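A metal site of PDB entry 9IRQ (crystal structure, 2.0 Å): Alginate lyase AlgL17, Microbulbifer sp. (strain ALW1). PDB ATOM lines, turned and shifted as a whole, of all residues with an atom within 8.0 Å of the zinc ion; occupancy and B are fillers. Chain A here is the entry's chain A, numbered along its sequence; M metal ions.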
ATOM      1  N   PRO A 281       9.479 -23.239 -15.361  1.00  0.00           N
ATOM      2  CA  PRO A 281       8.155 -22.619 -15.465  1.00  0.00           C
ATOM      3  C   PRO A 281       7.954 -21.731 -16.701  1.00  0.00           C
ATOM      4  O   PRO A 281       7.592 -20.605 -16.558  1.00  0.00           O
ATOM      5  CB  PRO A 281       8.094 -21.793 -14.175  1.00  0.00           C
ATOM      6  CG  PRO A 281       9.467 -21.290 -13.984  1.00  0.00           C
ATOM      7  CD  PRO A 281      10.265 -22.517 -14.343  1.00  0.00           C
ATOM      8  N   ILE A 282       8.199 -22.298 -17.869  1.00  0.00           N
ATOM      9  CA  ILE A 282       8.067 -21.529 -19.128  1.00  0.00           C
ATOM     10  C   ILE A 282       6.720 -21.837 -19.767  1.00  0.00           C
ATOM     11  O   ILE A 282       6.238 -22.950 -19.607  1.00  0.00           O
ATOM     12  CB  ILE A 282       9.254 -21.751 -20.086  1.00  0.00           C
ATOM     13  CG1 ILE A 282       9.326 -23.193 -20.572  1.00  0.00           C
ATOM     14  CG2 ILE A 282      10.566 -21.293 -19.450  1.00  0.00           C
ATOM     15  CD1 ILE A 282      10.458 -23.446 -21.518  1.00  0.00           C
ATOM     16  N   ASN A 283       6.155 -20.841 -20.424  1.00  0.00           N
ATOM     17  CA  ASN A 283       4.804 -20.987 -21.021  1.00  0.00           C
ATOM     18  C   ASN A 283       3.810 -21.114 -19.848  1.00  0.00           C
ATOM     19  O   ASN A 283       4.209 -20.822 -18.718  1.00  0.00           O
ATOM     20  CB  ASN A 283       4.757 -21.993 -22.159  1.00  0.00           C
ATOM     21  CG  ASN A 283       5.565 -21.612 -23.380  1.00  0.00           C
ATOM     22  OD1 ASN A 283       5.843 -20.446 -23.611  1.00  0.00           O
ATOM     23  ND2 ASN A 283       5.910 -22.595 -24.191  1.00  0.00           N
ATOM     24  N   ASP A 284       2.583 -21.517 -20.123  1.00  0.00           N
ATOM     25  CA  ASP A 284       1.617 -21.704 -19.029  1.00  0.00           C
ATOM     26  C   ASP A 284       2.212 -22.773 -18.142  1.00  0.00           C
ATOM     27  O   ASP A 284       2.504 -23.860 -18.655  1.00  0.00           O
ATOM     28  CB  ASP A 284       0.209 -21.998 -19.529  1.00  0.00           C
ATOM     29  CG  ASP A 284      -0.518 -20.759 -20.011  1.00  0.00           C
ATOM     30  OD1 ASP A 284      -0.077 -19.652 -19.686  1.00  0.00           O
ATOM     31  OD2 ASP A 284      -1.523 -20.898 -20.701  1.00  0.00           O
ATOM     32  N   ALA A 285       2.372 -22.443 -16.871  1.00  0.00           N
ATOM     33  CA  ALA A 285       3.036 -23.379 -15.965  1.00  0.00           C
ATOM     34  C   ALA A 285       2.758 -23.062 -14.496  1.00  0.00           C
ATOM     35  O   ALA A 285       2.726 -21.906 -14.133  1.00  0.00           O
ATOM     36  CB  ALA A 285       4.512 -23.409 -16.215  1.00  0.00           C
ATOM     37  N   LYS A 377      15.409 -19.250 -24.023  1.00  0.00           N
ATOM     38  CA  LYS A 377      14.200 -19.697 -24.710  1.00  0.00           C
ATOM     39  C   LYS A 377      14.026 -19.021 -26.069  1.00  0.00           C
ATOM     40  O   LYS A 377      13.099 -18.218 -26.265  1.00  0.00           O
ATOM     41  CB  LYS A 377      12.974 -19.485 -23.831  1.00  0.00           C
ATOM     42  CG  LYS A 377      11.730 -20.252 -24.283  1.00  0.00           C
ATOM     43  CD  LYS A 377      10.561 -20.022 -23.322  1.00  0.00           C
ATOM     44  CE  LYS A 377       9.248 -20.666 -23.833  1.00  0.00           C
ATOM     45  NZ  LYS A 377       8.477 -19.758 -24.759  1.00  0.00           N
ATOM     46  N   HIS A 385      -0.958 -22.046 -25.088  1.00  0.00           N
ATOM     47  CA  HIS A 385      -0.306 -21.879 -23.797  1.00  0.00           C
ATOM     48  C   HIS A 385       1.052 -21.190 -23.909  1.00  0.00           C
ATOM     49  O   HIS A 385       1.693 -20.928 -22.888  1.00  0.00           O
ATOM     50  CB  HIS A 385      -0.123 -23.241 -23.107  1.00  0.00           C
ATOM     51  CG  HIS A 385      -1.422 -23.867 -22.702  1.00  0.00           C
ATOM     52  ND1 HIS A 385      -2.251 -23.307 -21.759  1.00  0.00           N
ATOM     53  CD2 HIS A 385      -2.025 -25.004 -23.109  1.00  0.00           C
ATOM     54  CE1 HIS A 385      -3.324 -24.068 -21.620  1.00  0.00           C
ATOM     55  NE2 HIS A 385      -3.211 -25.103 -22.422  1.00  0.00           N
ATOM     56  N   GLY A 386       1.500 -20.896 -25.134  1.00  0.00           N
ATOM     57  CA  GLY A 386       2.774 -20.252 -25.289  1.00  0.00           C
ATOM     58  C   GLY A 386       2.751 -18.843 -24.737  1.00  0.00           C
ATOM     59  O   GLY A 386       1.736 -18.158 -24.732  1.00  0.00           O
ATOM     60  N   HIS A 387       3.908 -18.412 -24.234  1.00  0.00           N
ATOM     61  CA  HIS A 387       4.073 -17.034 -23.793  1.00  0.00           C
ATOM     62  C   HIS A 387       4.810 -16.218 -24.852  1.00  0.00           C
ATOM     63  O   HIS A 387       5.547 -16.761 -25.683  1.00  0.00           O
ATOM     64  CB  HIS A 387       4.811 -17.019 -22.456  1.00  0.00           C
ATOM     65  CG  HIS A 387       3.945 -17.487 -21.319  1.00  0.00           C
ATOM     66  ND1 HIS A 387       4.369 -17.502 -20.014  1.00  0.00           N
ATOM     67  CD2 HIS A 387       2.669 -17.930 -21.311  1.00  0.00           C
ATOM     68  CE1 HIS A 387       3.386 -17.951 -19.244  1.00  0.00           C
ATOM     69  NE2 HIS A 387       2.351 -18.218 -20.008  1.00  0.00           N
ATOM     70  N   PHE A 388       4.580 -14.897 -24.838  1.00  0.00           N
ATOM     71  CA  PHE A 388       5.162 -14.019 -25.866  1.00  0.00           C
ATOM     72  C   PHE A 388       6.520 -13.515 -25.370  1.00  0.00           C
ATOM     73  O   PHE A 388       6.676 -12.398 -24.890  1.00  0.00           O
ATOM     74  CB  PHE A 388       4.194 -12.886 -26.201  1.00  0.00           C
ATOM     75  CG  PHE A 388       2.921 -13.382 -26.834  1.00  0.00           C
ATOM     76  CD1 PHE A 388       1.840 -13.768 -26.041  1.00  0.00           C
ATOM     77  CD2 PHE A 388       2.804 -13.503 -28.203  1.00  0.00           C
ATOM     78  CE1 PHE A 388       0.669 -14.272 -26.600  1.00  0.00           C
ATOM     79  CE2 PHE A 388       1.643 -13.996 -28.782  1.00  0.00           C
ATOM     80  CZ  PHE A 388       0.557 -14.380 -27.969  1.00  0.00           C
ATOM     81  N   ASP A 389       7.519 -14.388 -25.500  1.00  0.00           N
ATOM     82  CA  ASP A 389       8.701 -14.275 -24.657  1.00  0.00           C
ATOM     83  C   ASP A 389       9.984 -14.627 -25.425  1.00  0.00           C
ATOM     84  O   ASP A 389      10.931 -15.174 -24.833  1.00  0.00           O
ATOM     85  CB  ASP A 389       8.533 -15.163 -23.407  1.00  0.00           C
ATOM     86  CG  ASP A 389       8.312 -16.645 -23.755  1.00  0.00           C
ATOM     87  OD1 ASP A 389       8.227 -16.986 -24.968  1.00  0.00           O
ATOM     88  OD2 ASP A 389       8.247 -17.493 -22.848  1.00  0.00           O
ATOM     89  N   THR A 392      13.758 -14.961 -24.065  1.00  0.00           N
ATOM     90  CA  THR A 392      13.808 -14.766 -22.627  1.00  0.00           C
ATOM     91  C   THR A 392      14.785 -15.741 -21.969  1.00  0.00           C
ATOM     92  O   THR A 392      15.171 -16.769 -22.550  1.00  0.00           O
ATOM     93  CB  THR A 392      12.435 -14.953 -21.980  1.00  0.00           C
ATOM     94  OG1 THR A 392      12.514 -14.551 -20.621  1.00  0.00           O
ATOM     95  CG2 THR A 392      12.018 -16.425 -22.031  1.00  0.00           C
ATOM     96  N   GLN A 394      16.165 -17.442 -17.880  1.00  0.00           N
ATOM     97  CA  GLN A 394      16.120 -17.597 -16.442  1.00  0.00           C
ATOM     98  C   GLN A 394      17.505 -17.977 -15.941  1.00  0.00           C
ATOM     99  O   GLN A 394      18.344 -18.481 -16.693  1.00  0.00           O
ATOM    100  CB  GLN A 394      15.167 -18.699 -16.002  1.00  0.00           C
ATOM    101  CG  GLN A 394      13.706 -18.415 -16.168  1.00  0.00           C
ATOM    102  CD  GLN A 394      12.944 -19.694 -16.068  1.00  0.00           C
ATOM    103  OE1 GLN A 394      12.385 -20.025 -15.016  1.00  0.00           O
ATOM    104  NE2 GLN A 394      12.946 -20.467 -17.141  1.00  0.00           N
ATOM    105  N   THR A 404      13.702 -14.806 -12.976  1.00  0.00           N
ATOM    106  CA  THR A 404      12.488 -15.614 -12.933  1.00  0.00           C
ATOM    107  C   THR A 404      11.599 -15.483 -14.165  1.00  0.00           C
ATOM    108  O   THR A 404      11.613 -14.487 -14.894  1.00  0.00           O
ATOM    109  CB  THR A 404      11.660 -15.257 -11.689  1.00  0.00           C
ATOM    110  OG1 THR A 404      11.246 -13.884 -11.791  1.00  0.00           O
ATOM    111  CG2 THR A 404      12.519 -15.400 -10.452  1.00  0.00           C
ATOM    112  N   ASP A 405      10.813 -16.534 -14.363  1.00  0.00           N
ATOM    113  CA  ASP A 405       9.661 -16.570 -15.271  1.00  0.00           C
ATOM    114  C   ASP A 405       8.412 -16.715 -14.407  1.00  0.00           C
ATOM    115  O   ASP A 405       8.380 -17.561 -13.504  1.00  0.00           O
ATOM    116  CB  ASP A 405       9.772 -17.769 -16.220  1.00  0.00           C
ATOM    117  CG  ASP A 405       8.960 -17.594 -17.502  1.00  0.00           C
ATOM    118  OD1 ASP A 405       7.912 -16.941 -17.480  1.00  0.00           O
ATOM    119  OD2 ASP A 405       9.381 -18.157 -18.531  1.00  0.00           O
ATOM    120  N   TYR A 406       7.388 -15.891 -14.678  1.00  0.00           N
ATOM    121  CA  TYR A 406       6.199 -15.915 -13.836  1.00  0.00           C
ATOM    122  C   TYR A 406       5.460 -17.246 -13.879  1.00  0.00           C
ATOM    123  O   TYR A 406       4.813 -17.629 -12.891  1.00  0.00           O
ATOM    124  CB  TYR A 406       5.238 -14.795 -14.250  1.00  0.00           C
ATOM    125  CG  TYR A 406       4.189 -14.547 -13.184  1.00  0.00           C
ATOM    126  CD1 TYR A 406       4.476 -13.734 -12.086  1.00  0.00           C
ATOM    127  CD2 TYR A 406       2.918 -15.147 -13.249  1.00  0.00           C
ATOM    128  CE1 TYR A 406       3.530 -13.514 -11.097  1.00  0.00           C
ATOM    129  CE2 TYR A 406       1.955 -14.920 -12.244  1.00  0.00           C
ATOM    130  CZ  TYR A 406       2.272 -14.112 -11.181  1.00  0.00           C
ATOM    131  OH  TYR A 406       1.349 -13.900 -10.176  1.00  0.00           O
ATOM    132  N   GLY A 407       5.537 -17.974 -14.992  1.00  0.00           N
ATOM    133  CA  GLY A 407       4.570 -19.057 -15.081  1.00  0.00           C
ATOM    134  C   GLY A 407       3.170 -18.505 -15.358  1.00  0.00           C
ATOM    135  O   GLY A 407       2.989 -17.378 -15.794  1.00  0.00           O
ATOM    136  N   ALA A 408       2.169 -19.327 -15.073  1.00  0.00           N
ATOM    137  CA  ALA A 408       0.795 -18.936 -15.326  1.00  0.00           C
ATOM    138  C   ALA A 408       0.182 -18.202 -14.142  1.00  0.00           C
ATOM    139  O   ALA A 408       0.554 -18.415 -12.990  1.00  0.00           O
ATOM    140  CB  ALA A 408      -0.057 -20.163 -15.652  1.00  0.00           C
ATOM    141  N   ASN A 426      -3.765 -14.130 -16.609  1.00  0.00           N
ATOM    142  CA  ASN A 426      -2.850 -14.954 -17.400  1.00  0.00           C
ATOM    143  C   ASN A 426      -2.690 -14.364 -18.792  1.00  0.00           C
ATOM    144  O   ASN A 426      -1.606 -14.373 -19.365  1.00  0.00           O
ATOM    145  CB  ASN A 426      -3.344 -16.389 -17.493  1.00  0.00           C
ATOM    146  CG  ASN A 426      -2.242 -17.335 -17.922  1.00  0.00           C
ATOM    147  OD1 ASN A 426      -1.253 -17.485 -17.202  1.00  0.00           O
ATOM    148  ND2 ASN A 426      -2.404 -17.987 -19.084  1.00  0.00           N
ATOM    149  N   TRP A 429      -1.278 -10.357 -18.053  1.00  0.00           N
ATOM    150  CA  TRP A 429       0.050 -10.256 -17.465  1.00  0.00           C
ATOM    151  C   TRP A 429       0.968 -11.403 -17.900  1.00  0.00           C
ATOM    152  O   TRP A 429       1.999 -11.151 -18.544  1.00  0.00           O
ATOM    153  CB  TRP A 429      -0.026 -10.206 -15.934  1.00  0.00           C
ATOM    154  CG  TRP A 429       1.303 -10.461 -15.305  1.00  0.00           C
ATOM    155  CD1 TRP A 429       1.677 -11.586 -14.612  1.00  0.00           C
ATOM    156  CD2 TRP A 429       2.458  -9.599 -15.335  1.00  0.00           C
ATOM    157  NE1 TRP A 429       3.003 -11.467 -14.202  1.00  0.00           N
ATOM    158  CE2 TRP A 429       3.497 -10.262 -14.638  1.00  0.00           C
ATOM    159  CE3 TRP A 429       2.701  -8.329 -15.853  1.00  0.00           C
ATOM    160  CZ2 TRP A 429       4.766  -9.696 -14.466  1.00  0.00           C
ATOM    161  CZ3 TRP A 429       3.964  -7.768 -15.692  1.00  0.00           C
ATOM    162  CH2 TRP A 429       4.980  -8.453 -14.997  1.00  0.00           C
ATOM    163  N   ALA A 430       0.629 -12.642 -17.571  1.00  0.00           N
ATOM    164  CA  ALA A 430       1.621 -13.720 -17.555  1.00  0.00           C
ATOM    165  C   ALA A 430       2.130 -14.056 -18.952  1.00  0.00           C
ATOM    166  O   ALA A 430       3.285 -14.460 -19.114  1.00  0.00           O
ATOM    167  CB  ALA A 430       1.040 -14.959 -16.887  1.00  0.00           C
ATOM    168  N   LYS A 431       1.279 -13.910 -19.971  1.00  0.00           N
ATOM    169  CA  LYS A 431       1.680 -14.166 -21.348  1.00  0.00           C
ATOM    170  C   LYS A 431       2.450 -13.013 -21.967  1.00  0.00           C
ATOM    171  O   LYS A 431       3.116 -13.193 -22.989  1.00  0.00           O
ATOM    172  CB  LYS A 431       0.426 -14.463 -22.186  1.00  0.00           C
ATOM    173  CG  LYS A 431      -0.059 -15.876 -21.970  1.00  0.00           C
ATOM    174  CD  LYS A 431      -1.387 -16.172 -22.700  1.00  0.00           C
ATOM    175  CE  LYS A 431      -1.585 -17.679 -22.835  1.00  0.00           C
ATOM    176  NZ  LYS A 431      -2.686 -18.002 -23.791  1.00  0.00           N
ATOM    177  N   GLN A 432       2.390 -11.837 -21.345  1.00  0.00           N
ATOM    178  CA  GLN A 432       2.915 -10.635 -21.969  1.00  0.00           C
ATOM    179  C   GLN A 432       4.431 -10.586 -21.861  1.00  0.00           C
ATOM    180  O   GLN A 432       5.046 -11.129 -20.938  1.00  0.00           O
ATOM    181  CB  GLN A 432       2.263  -9.404 -21.354  1.00  0.00           C
ATOM    182  CG  GLN A 432       0.737  -9.390 -21.514  1.00  0.00           C
ATOM    183  CD  GLN A 432       0.297  -9.457 -22.967  1.00  0.00           C
ATOM    184  OE1 GLN A 432       0.831  -8.752 -23.820  1.00  0.00           O
ATOM    185  NE2 GLN A 432      -0.661 -10.323 -23.254  1.00  0.00           N
ATOM    186  N   ALA A 435       6.332  -9.322 -18.849  1.00  0.00           N
ATOM    187  CA  ALA A 435       6.466 -10.225 -17.708  1.00  0.00           C
ATOM    188  C   ALA A 435       7.705 -11.122 -17.806  1.00  0.00           C
ATOM    189  O   ALA A 435       7.902 -11.935 -16.899  1.00  0.00           O
ATOM    190  CB  ALA A 435       5.202 -11.078 -17.568  1.00  0.00           C
ATOM    191  N   HIS A 436       8.543 -10.974 -18.829  1.00  0.00           N
ATOM    192  CA  HIS A 436       9.677 -11.865 -19.052  1.00  0.00           C
ATOM    193  C   HIS A 436      10.959 -11.047 -19.133  1.00  0.00           C
ATOM    194  O   HIS A 436      10.929  -9.817 -19.066  1.00  0.00           O
ATOM    195  CB  HIS A 436       9.470 -12.699 -20.316  1.00  0.00           C
ATOM    196  CG  HIS A 436       8.251 -13.557 -20.237  1.00  0.00           C
ATOM    197  ND1 HIS A 436       6.994 -13.076 -20.507  1.00  0.00           N
ATOM    198  CD2 HIS A 436       8.095 -14.844 -19.874  1.00  0.00           C
ATOM    199  CE1 HIS A 436       6.104 -14.036 -20.316  1.00  0.00           C
ATOM    200  NE2 HIS A 436       6.752 -15.119 -19.931  1.00  0.00           N
ATOM    201  N   ASN A 437      12.091 -11.751 -19.255  1.00  0.00           N
ATOM    202  CA  ASN A 437      13.413 -11.120 -19.254  1.00  0.00           C
ATOM    203  C   ASN A 437      13.927 -11.019 -20.690  1.00  0.00           C
ATOM    204  O   ASN A 437      14.878 -11.685 -21.112  1.00  0.00           O
ATOM    205  CB  ASN A 437      14.375 -11.899 -18.365  1.00  0.00           C
ATOM    206  CG  ASN A 437      13.824 -12.101 -16.966  1.00  0.00           C
ATOM    207  OD1 ASN A 437      13.457 -11.138 -16.312  1.00  0.00           O
ATOM    208  ND2 ASN A 437      13.771 -13.356 -16.503  1.00  0.00           N
HETATM  209 ZN    ZN M   1       6.229 -17.063 -18.994  1.00  0.00          ZN
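The backbone carbonyl oxygen (O) of Ala 430 lies close to a ring nitrogen (ND1) of His 387, at 3.4 Å. The backbone NH (N) of His 387 lies within hydrogen-bond range of the side-chain amide oxygen (OD1) of Asn 283. A ring nitrogen (NE2) of His 387 is in hydrogen-bond range of the side-chain carboxylate of Asp 284 (2.8 Å). ND1 of His 436 lies within hydrogen-bond range of O of Gln 432 (2.8 Å).
Residues that only touch the zinc ion: Ala 430 (3.9 Å). The nearest printed residue that does not touch the zinc ion is Asn 283 (4.04 Å).
ND1 of His 387 binds the zinc ion (2.2 Å). The zinc ion is bound by a ring nitrogen (NE2) of His 436 (2.2 Å). OD1 of Asp 405 is bound to the zinc ion (2.3 Å).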
